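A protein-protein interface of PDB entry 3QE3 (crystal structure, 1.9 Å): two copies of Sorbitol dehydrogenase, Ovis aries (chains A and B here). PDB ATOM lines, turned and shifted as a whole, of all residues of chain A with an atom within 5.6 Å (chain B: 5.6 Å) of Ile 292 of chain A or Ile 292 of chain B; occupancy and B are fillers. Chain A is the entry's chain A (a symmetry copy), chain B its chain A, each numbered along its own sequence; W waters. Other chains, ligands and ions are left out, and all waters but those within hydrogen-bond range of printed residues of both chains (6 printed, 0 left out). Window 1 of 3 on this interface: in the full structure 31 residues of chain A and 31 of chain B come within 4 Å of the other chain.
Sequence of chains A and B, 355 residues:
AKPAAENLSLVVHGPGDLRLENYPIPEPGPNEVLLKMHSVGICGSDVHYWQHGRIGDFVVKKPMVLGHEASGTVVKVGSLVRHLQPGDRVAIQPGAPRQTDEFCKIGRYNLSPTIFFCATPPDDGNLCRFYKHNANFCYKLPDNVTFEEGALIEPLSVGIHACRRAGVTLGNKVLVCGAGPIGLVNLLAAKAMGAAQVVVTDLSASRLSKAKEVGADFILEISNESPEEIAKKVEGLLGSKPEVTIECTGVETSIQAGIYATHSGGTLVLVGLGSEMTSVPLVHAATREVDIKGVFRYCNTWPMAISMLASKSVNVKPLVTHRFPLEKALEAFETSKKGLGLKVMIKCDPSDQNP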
ATOM      1  N   ILE A 259     -35.123  22.759   5.317  1.00  0.00           N
ATOM      2  CA  ILE A 259     -35.562  24.146   5.328  1.00  0.00           C
ATOM      3  C   ILE A 259     -37.078  24.281   5.151  1.00  0.00           C
ATOM      4  O   ILE A 259     -37.734  25.046   5.868  1.00  0.00           O
ATOM      5  CB  ILE A 259     -34.785  24.966   4.270  1.00  0.00           C
ATOM      6  CG1 ILE A 259     -33.297  24.981   4.657  1.00  0.00           C
ATOM      7  CG2 ILE A 259     -35.380  26.360   4.131  1.00  0.00           C
ATOM      8  CD1 ILE A 259     -32.398  25.829   3.773  1.00  0.00           C
ATOM      9  N   THR A 267     -35.141  25.359  14.258  1.00  0.00           N
ATOM     10  CA  THR A 267     -33.725  25.235  13.955  1.00  0.00           C
ATOM     11  C   THR A 267     -33.386  23.994  13.114  1.00  0.00           C
ATOM     12  O   THR A 267     -33.802  22.870  13.420  1.00  0.00           O
ATOM     13  CB  THR A 267     -32.892  25.163  15.247  1.00  0.00           C
ATOM     14  OG1 THR A 267     -33.104  26.343  16.039  1.00  0.00           O
ATOM     15  CG2 THR A 267     -31.421  25.020  14.915  1.00  0.00           C
ATOM     16  N   LEU A 268     -32.619  24.218  12.058  1.00  0.00           N
ATOM     17  CA  LEU A 268     -32.052  23.167  11.236  1.00  0.00           C
ATOM     18  C   LEU A 268     -30.567  23.084  11.549  1.00  0.00           C
ATOM     19  O   LEU A 268     -29.835  24.068  11.405  1.00  0.00           O
ATOM     20  CB  LEU A 268     -32.234  23.512   9.751  1.00  0.00           C
ATOM     21  CG  LEU A 268     -31.405  22.702   8.759  1.00  0.00           C
ATOM     22  CD1 LEU A 268     -31.867  21.238   8.747  1.00  0.00           C
ATOM     23  CD2 LEU A 268     -31.531  23.288   7.365  1.00  0.00           C
ATOM     24  N   LEU A 270     -27.007  21.169  10.651  1.00  0.00           N
ATOM     25  CA  LEU A 270     -26.317  20.460   9.592  1.00  0.00           C
ATOM     26  C   LEU A 270     -25.197  19.641  10.213  1.00  0.00           C
ATOM     27  O   LEU A 270     -24.241  20.193  10.749  1.00  0.00           O
ATOM     28  CB  LEU A 270     -25.745  21.474   8.591  1.00  0.00           C
ATOM     29  CG  LEU A 270     -26.783  22.465   8.044  1.00  0.00           C
ATOM     30  CD1 LEU A 270     -26.190  23.468   7.057  1.00  0.00           C
ATOM     31  CD2 LEU A 270     -27.953  21.723   7.411  1.00  0.00           C
ATOM     32  N   LEU A 282     -32.275  29.830   1.029  1.00  0.00           N
ATOM     33  CA  LEU A 282     -31.804  30.571   2.184  1.00  0.00           C
ATOM     34  C   LEU A 282     -32.861  31.559   2.641  1.00  0.00           C
ATOM     35  O   LEU A 282     -33.134  31.692   3.835  1.00  0.00           O
ATOM     36  CB  LEU A 282     -30.516  31.307   1.826  1.00  0.00           C
ATOM     37  CG  LEU A 282     -29.678  31.806   2.985  1.00  0.00           C
ATOM     38  CD1 LEU A 282     -29.630  30.764   4.089  1.00  0.00           C
ATOM     39  CD2 LEU A 282     -28.278  32.179   2.499  1.00  0.00           C
ATOM     40  N   ALA A 285     -35.956  29.983   4.639  1.00  0.00           N
ATOM     41  CA  ALA A 285     -35.583  29.833   6.047  1.00  0.00           C
ATOM     42  C   ALA A 285     -35.522  31.151   6.789  1.00  0.00           C
ATOM     43  O   ALA A 285     -36.072  31.290   7.885  1.00  0.00           O
ATOM     44  CB  ALA A 285     -34.252  29.103   6.170  1.00  0.00           C
ATOM     45  N   VAL A 290     -36.147  30.377  10.637  1.00  0.00           N
ATOM     46  CA  VAL A 290     -35.538  29.050  10.822  1.00  0.00           C
ATOM     47  C   VAL A 290     -34.038  29.254  10.834  1.00  0.00           C
ATOM     48  O   VAL A 290     -33.448  29.644   9.822  1.00  0.00           O
ATOM     49  CB  VAL A 290     -35.911  28.074   9.679  1.00  0.00           C
ATOM     50  CG1 VAL A 290     -35.277  26.688   9.896  1.00  0.00           C
ATOM     51  CG2 VAL A 290     -37.433  27.953   9.540  1.00  0.00           C
ATOM     52  N   ASP A 291     -33.413  29.011  11.977  1.00  0.00           N
ATOM     53  CA  ASP A 291     -31.975  29.157  12.069  1.00  0.00           C
ATOM     54  C   ASP A 291     -31.275  27.989  11.404  1.00  0.00           C
ATOM     55  O   ASP A 291     -31.755  26.850  11.434  1.00  0.00           O
ATOM     56  CB  ASP A 291     -31.526  29.265  13.524  1.00  0.00           C
ATOM     57  CG  ASP A 291     -32.055  30.526  14.194  1.00  0.00           C
ATOM     58  OD1 ASP A 291     -32.406  31.476  13.470  1.00  0.00           O
ATOM     59  OD2 ASP A 291     -32.114  30.565  15.431  1.00  0.00           O
ATOM     60  N   ILE A 292     -30.120  28.272  10.824  1.00  0.00           N
ATOM     61  CA  ILE A 292     -29.319  27.225  10.245  1.00  0.00           C
ATOM     62  C   ILE A 292     -28.002  27.176  10.983  1.00  0.00           C
ATOM     63  O   ILE A 292     -27.227  28.130  10.936  1.00  0.00           O
ATOM     64  CB  ILE A 292     -29.079  27.476   8.763  1.00  0.00           C
ATOM     65  CG1 ILE A 292     -30.412  27.443   8.015  1.00  0.00           C
ATOM     66  CG2 ILE A 292     -28.119  26.430   8.212  1.00  0.00           C
ATOM     67  CD1 ILE A 292     -30.336  27.935   6.572  1.00  0.00           C
ATOM     68  N   LYS A 293     -27.763  26.061  11.672  1.00  0.00           N
ATOM     69  CA  LYS A 293     -26.583  25.896  12.506  1.00  0.00           C
ATOM     70  C   LYS A 293     -25.797  24.688  12.046  1.00  0.00           C
ATOM     71  O   LYS A 293     -26.370  23.713  11.558  1.00  0.00           O
ATOM     72  CB  LYS A 293     -26.990  25.681  13.974  1.00  0.00           C
ATOM     73  CG  LYS A 293     -27.663  26.874  14.595  1.00  0.00           C
ATOM     74  CD  LYS A 293     -27.783  26.699  16.108  1.00  0.00           C
ATOM     75  CE  LYS A 293     -28.441  27.906  16.741  1.00  0.00           C
ATOM     76  NZ  LYS A 293     -28.509  27.735  18.211  1.00  0.00           N
ATOM     77  N   GLY A 294     -24.484  24.745  12.217  1.00  0.00           N
ATOM     78  CA  GLY A 294     -23.646  23.607  11.903  1.00  0.00           C
ATOM     79  C   GLY A 294     -23.081  23.046  13.184  1.00  0.00           C
ATOM     80  O   GLY A 294     -23.414  23.502  14.274  1.00  0.00           O
ATOM     81  N   ILE B 259     -19.914  34.921   5.541  1.00  0.00           N
ATOM     82  CA  ILE B 259     -19.528  33.592   5.992  1.00  0.00           C
ATOM     83  C   ILE B 259     -18.016  33.461   6.201  1.00  0.00           C
ATOM     84  O   ILE B 259     -17.561  32.916   7.213  1.00  0.00           O
ATOM     85  CB  ILE B 259     -20.070  32.515   5.022  1.00  0.00           C
ATOM     86  CG1 ILE B 259     -21.607  32.553   5.055  1.00  0.00           C
ATOM     87  CG2 ILE B 259     -19.499  31.147   5.368  1.00  0.00           C
ATOM     88  CD1 ILE B 259     -22.307  31.488   4.227  1.00  0.00           C
ATOM     89  N   THR B 267     -21.988  34.605  14.614  1.00  0.00           N
ATOM     90  CA  THR B 267     -23.295  34.610  13.977  1.00  0.00           C
ATOM     91  C   THR B 267     -23.400  35.595  12.802  1.00  0.00           C
ATOM     92  O   THR B 267     -23.031  36.772  12.908  1.00  0.00           O
ATOM     93  CB  THR B 267     -24.396  34.974  14.989  1.00  0.00           C
ATOM     94  OG1 THR B 267     -24.402  34.032  16.075  1.00  0.00           O
ATOM     95  CG2 THR B 267     -25.750  34.989  14.310  1.00  0.00           C
ATOM     96  N   LEU B 268     -23.915  35.096  11.689  1.00  0.00           N
ATOM     97  CA  LEU B 268     -24.252  35.896  10.528  1.00  0.00           C
ATOM     98  C   LEU B 268     -25.767  36.011  10.467  1.00  0.00           C
ATOM     99  O   LEU B 268     -26.475  35.001  10.409  1.00  0.00           O
ATOM    100  CB  LEU B 268     -23.749  35.201   9.254  1.00  0.00           C
ATOM    101  CG  LEU B 268     -24.310  35.717   7.932  1.00  0.00           C
ATOM    102  CD1 LEU B 268     -23.815  37.146   7.664  1.00  0.00           C
ATOM    103  CD2 LEU B 268     -23.890  34.810   6.791  1.00  0.00           C
ATOM    104  N   LEU B 270     -28.975  37.542   8.346  1.00  0.00           N
ATOM    105  CA  LEU B 270     -29.389  37.949   7.018  1.00  0.00           C
ATOM    106  C   LEU B 270     -30.595  38.863   7.148  1.00  0.00           C
ATOM    107  O   LEU B 270     -31.664  38.433   7.574  1.00  0.00           O
ATOM    108  CB  LEU B 270     -29.748  36.704   6.194  1.00  0.00           C
ATOM    109  CG  LEU B 270     -28.643  35.639   6.157  1.00  0.00           C
ATOM    110  CD1 LEU B 270     -29.026  34.407   5.341  1.00  0.00           C
ATOM    111  CD2 LEU B 270     -27.339  36.235   5.642  1.00  0.00           C
ATOM    112  N   LEU B 282     -21.923  26.933   2.599  1.00  0.00           N
ATOM    113  CA  LEU B 282     -22.663  26.486   3.764  1.00  0.00           C
ATOM    114  C   LEU B 282     -21.764  25.672   4.676  1.00  0.00           C
ATOM    115  O   LEU B 282     -21.773  25.845   5.896  1.00  0.00           O
ATOM    116  CB  LEU B 282     -23.857  25.648   3.317  1.00  0.00           C
ATOM    117  CG  LEU B 282     -24.949  25.426   4.343  1.00  0.00           C
ATOM    118  CD1 LEU B 282     -25.215  26.706   5.116  1.00  0.00           C
ATOM    119  CD2 LEU B 282     -26.213  24.905   3.661  1.00  0.00           C
ATOM    120  N   ALA B 285     -19.156  27.779   6.870  1.00  0.00           N
ATOM    121  CA  ALA B 285     -19.834  28.260   8.076  1.00  0.00           C
ATOM    122  C   ALA B 285     -20.098  27.165   9.086  1.00  0.00           C
ATOM    123  O   ALA B 285     -19.814  27.316  10.278  1.00  0.00           O
ATOM    124  CB  ALA B 285     -21.137  28.960   7.712  1.00  0.00           C
ATOM    125  N   VAL B 290     -20.336  28.881  12.663  1.00  0.00           N
ATOM    126  CA  VAL B 290     -20.932  30.194  12.373  1.00  0.00           C
ATOM    127  C   VAL B 290     -22.402  29.957  12.097  1.00  0.00           C
ATOM    128  O   VAL B 290     -22.759  29.313  11.105  1.00  0.00           O
ATOM    129  CB  VAL B 290     -20.284  30.869  11.140  1.00  0.00           C
ATOM    130  CG1 VAL B 290     -20.909  32.246  10.860  1.00  0.00           C
ATOM    131  CG2 VAL B 290     -18.766  30.995  11.322  1.00  0.00           C
ATOM    132  N   ASP B 291     -23.261  30.455  12.973  1.00  0.00           N
ATOM    133  CA  ASP B 291     -24.686  30.295  12.771  1.00  0.00           C
ATOM    134  C   ASP B 291     -25.184  31.243  11.699  1.00  0.00           C
ATOM    135  O   ASP B 291     -24.691  32.368  11.555  1.00  0.00           O
ATOM    136  CB  ASP B 291     -25.455  30.536  14.067  1.00  0.00           C
ATOM    137  CG  ASP B 291     -25.127  29.495  15.129  1.00  0.00           C
ATOM    138  OD1 ASP B 291     -24.648  28.406  14.760  1.00  0.00           O
ATOM    139  OD2 ASP B 291     -25.349  29.764  16.319  1.00  0.00           O
ATOM    140  N   ILE B 292     -26.186  30.793  10.962  1.00  0.00           N
ATOM    141  CA  ILE B 292     -26.806  31.642   9.976  1.00  0.00           C
ATOM    142  C   ILE B 292     -28.253  31.834  10.363  1.00  0.00           C
ATOM    143  O   ILE B 292     -29.025  30.876  10.379  1.00  0.00           O
ATOM    144  CB  ILE B 292     -26.713  31.027   8.588  1.00  0.00           C
ATOM    145  CG1 ILE B 292     -25.245  30.913   8.175  1.00  0.00           C
ATOM    146  CG2 ILE B 292     -27.492  31.877   7.594  1.00  0.00           C
ATOM    147  CD1 ILE B 292     -25.007  30.078   6.920  1.00  0.00           C
ATOM    148  N   LYS B 293     -28.609  33.077  10.684  1.00  0.00           N
ATOM    149  CA  LYS B 293     -29.943  33.408  11.163  1.00  0.00           C
ATOM    150  C   LYS B 293     -30.569  34.443  10.255  1.00  0.00           C
ATOM    151  O   LYS B 293     -29.873  35.284   9.684  1.00  0.00           O
ATOM    152  CB  LYS B 293     -29.871  33.990  12.586  1.00  0.00           C
ATOM    153  CG  LYS B 293     -29.390  33.006  13.617  1.00  0.00           C
ATOM    154  CD  LYS B 293     -29.609  33.552  15.027  1.00  0.00           C
ATOM    155  CE  LYS B 293     -29.146  32.557  16.069  1.00  0.00           C
ATOM    156  NZ  LYS B 293     -29.407  33.087  17.428  1.00  0.00           N
ATOM    157  N   GLY B 294     -31.888  34.392  10.133  1.00  0.00           N
ATOM    158  CA  GLY B 294     -32.601  35.393   9.368  1.00  0.00           C
ATOM    159  C   GLY B 294     -33.424  36.236  10.309  1.00  0.00           C
ATOM    160  O   GLY B 294     -33.359  36.072  11.525  1.00  0.00           O
HETATM  161  O   HOH W   1     -31.273  31.084   8.562  1.00  0.00           O
HETATM  162  O   HOH W   2     -32.259  32.404  17.438  1.00  0.00           O
HETATM  163  O   HOH W   3     -33.386  32.242  11.085  1.00  0.00           O
HETATM  164  O   HOH W   4     -24.634  27.545   9.782  1.00  0.00           O
HETATM  165  O   HOH W   5     -25.714  28.481  18.696  1.00  0.00           O
HETATM  166  O   HOH W   6     -23.178  27.105  12.922  1.00  0.00           O
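Of chain B, only Asp 291 (3.8 Å) and Ile 292 (2.9 Å) come within 4 Å of Ile 292 of chain A.
Ile 292 of chain B touches just these residues of chain A: Asp 291 (3.8 Å) and Ile 292 (2.9 Å).
Of the printed residues of chain B, Leu 270 of chain A touches Leu 282.
Printed residues of chain A within 4 Å of Asp 291 of chain B: Ile 292 (3.8 Å) and Lys 293 (3.4 Å).
Of the printed residues of chain B, Lys 293 of chain A touches Asp 291.
Of the printed residues of chain A, Lys 293 of chain B touches Asp 291 (3.4 Å).
Printed residues of chain A within 4 Å of Leu 282 of chain B: Leu 270 (3.6 Å).
The nearest residue of chain B that does not touch Ile 292 of chain A is Leu 282 of chain B (4.3 Å).
The nearest printed residue of chain B that does not touch Lys 293 of chain A is Lys 293 of chain B (4.8 Å).
Water W6 lies within hydrogen-bond range of the side-chain carboxylate of Asp 291 of chain B (2.7 Å), the backbone NH of Gly 294 of chain A (2.8 Å) and the backbone carbonyl oxygen of Val 290 of chain B (2.9 Å).
Water W3 lies within hydrogen-bond range of the side-chain carboxylate (OD1) of Asp 291 of chain A (2.7 Å), the backbone NH (N) of Gly 294 of chain B (2.8 Å) and the backbone carbonyl oxygen (O) of Val 290 of chain A (2.9 Å).
Water W5 bridges the side-chain carboxylate (OD2) of Asp 291 of chain B (2.7 Å) and the side-chain amino group (NZ) of Lys 293 of chain A (2.9 Å).
Water W2 lies within hydrogen-bond range of the side-chain carboxylate of Asp 291 of chain A (2.7 Å) and the side-chain amino group of Lys 293 of chain B (2.9 Å).
Water W1 lies within hydrogen-bond range of the backbone carbonyl oxygen of Val 290 of chain A (2.9 Å) and the backbone carbonyl oxygen of Ile 292 of chain B (2.9 Å).
Water W4 bridges O of Val 290 of chain B (2.9 Å) and O of Ile 292 of chain A (2.9 Å).
The backbone NH (N) of Leu 268 of chain B sits at hydrogen-bond distance from the backbone carbonyl oxygen (O) of Asp 291 of chain B (2.8 Å).
O of Leu 268 of chain B sits at hydrogen-bond distance from N of Lys 293 of chain B (2.9 Å).
The backbone carbonyl oxygen (O) of Lys 293 of chain B is in hydrogen-bond range of the backbone NH (N) of Leu 270 of chain B (2.8 Å).
The backbone NH (N) of Leu 268 of chain A sits at hydrogen-bond distance from the backbone carbonyl oxygen (O) of Asp 291 of chain A.
The backbone carbonyl oxygen (O) of Leu 268 of chain A is in hydrogen-bond range of the backbone NH (N) of Lys 293 of chain A, 2.9 Å away.
The backbone NH of Leu 270 of chain A is in hydrogen-bond range of the backbone carbonyl oxygen of Lys 293 of chain A (2.8 Å).
Among the printed residues, merely in contact across the chains: Asp 291 of chain A with Lys 293 of chain B (3.4 Å), Lys 293 of chain A with Asp 291 of chain B (3.4 Å), Leu 270 of chain A with Leu 282 of chain B (3.6 Å), Leu 282 of chain A with Leu 270 of chain B (3.6 Å), Ile 292 of chain A with Asp 291 of chain B (3.8 Å) and Asp 291 of chain A with Ile 292 of chain B (3.8 Å).
Of the 11 printed residues of chain A, 5 touch a printed residue of chain B.
Of the 11 printed residues of chain B, 5 touch a printed residue of chain A.
Hydrophobic or aromatic side chains of chain B that line the printed part of chain A: Leu 270, Leu 282 and Ile 292.
Along chain B the printed residues that touch a printed residue of chain A span positions 270 to 293.
Among the printed residues, no Asp or Glu carboxylate lies within 4 Å of a Lys or Arg side-chain nitrogen of the other chain.
N of Ile 292 of chain B sits at hydrogen-bond distance from O of Ile 292 of chain A.
Leu 270 of chain A touches Leu 282 of chain B, and with the chains exchanged Leu 282 of chain A touches Leu 270 of chain B.
Asp 291 of chain A touches Ile 292 of chain B, and with the chains exchanged Ile 292 of chain A touches Asp 291 of chain B.
Asp 291 of chain A touches Lys 293 of chain B, and with the chains exchanged Lys 293 of chain A touches Asp 291 of chain B.
Ile 292 of chain A touches its own counterpart, Ile 292 of chain B.
Positions printed for both chains: 259, 267, 268, 270, 282, 285, 290, 291, 292, 293 and 294.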
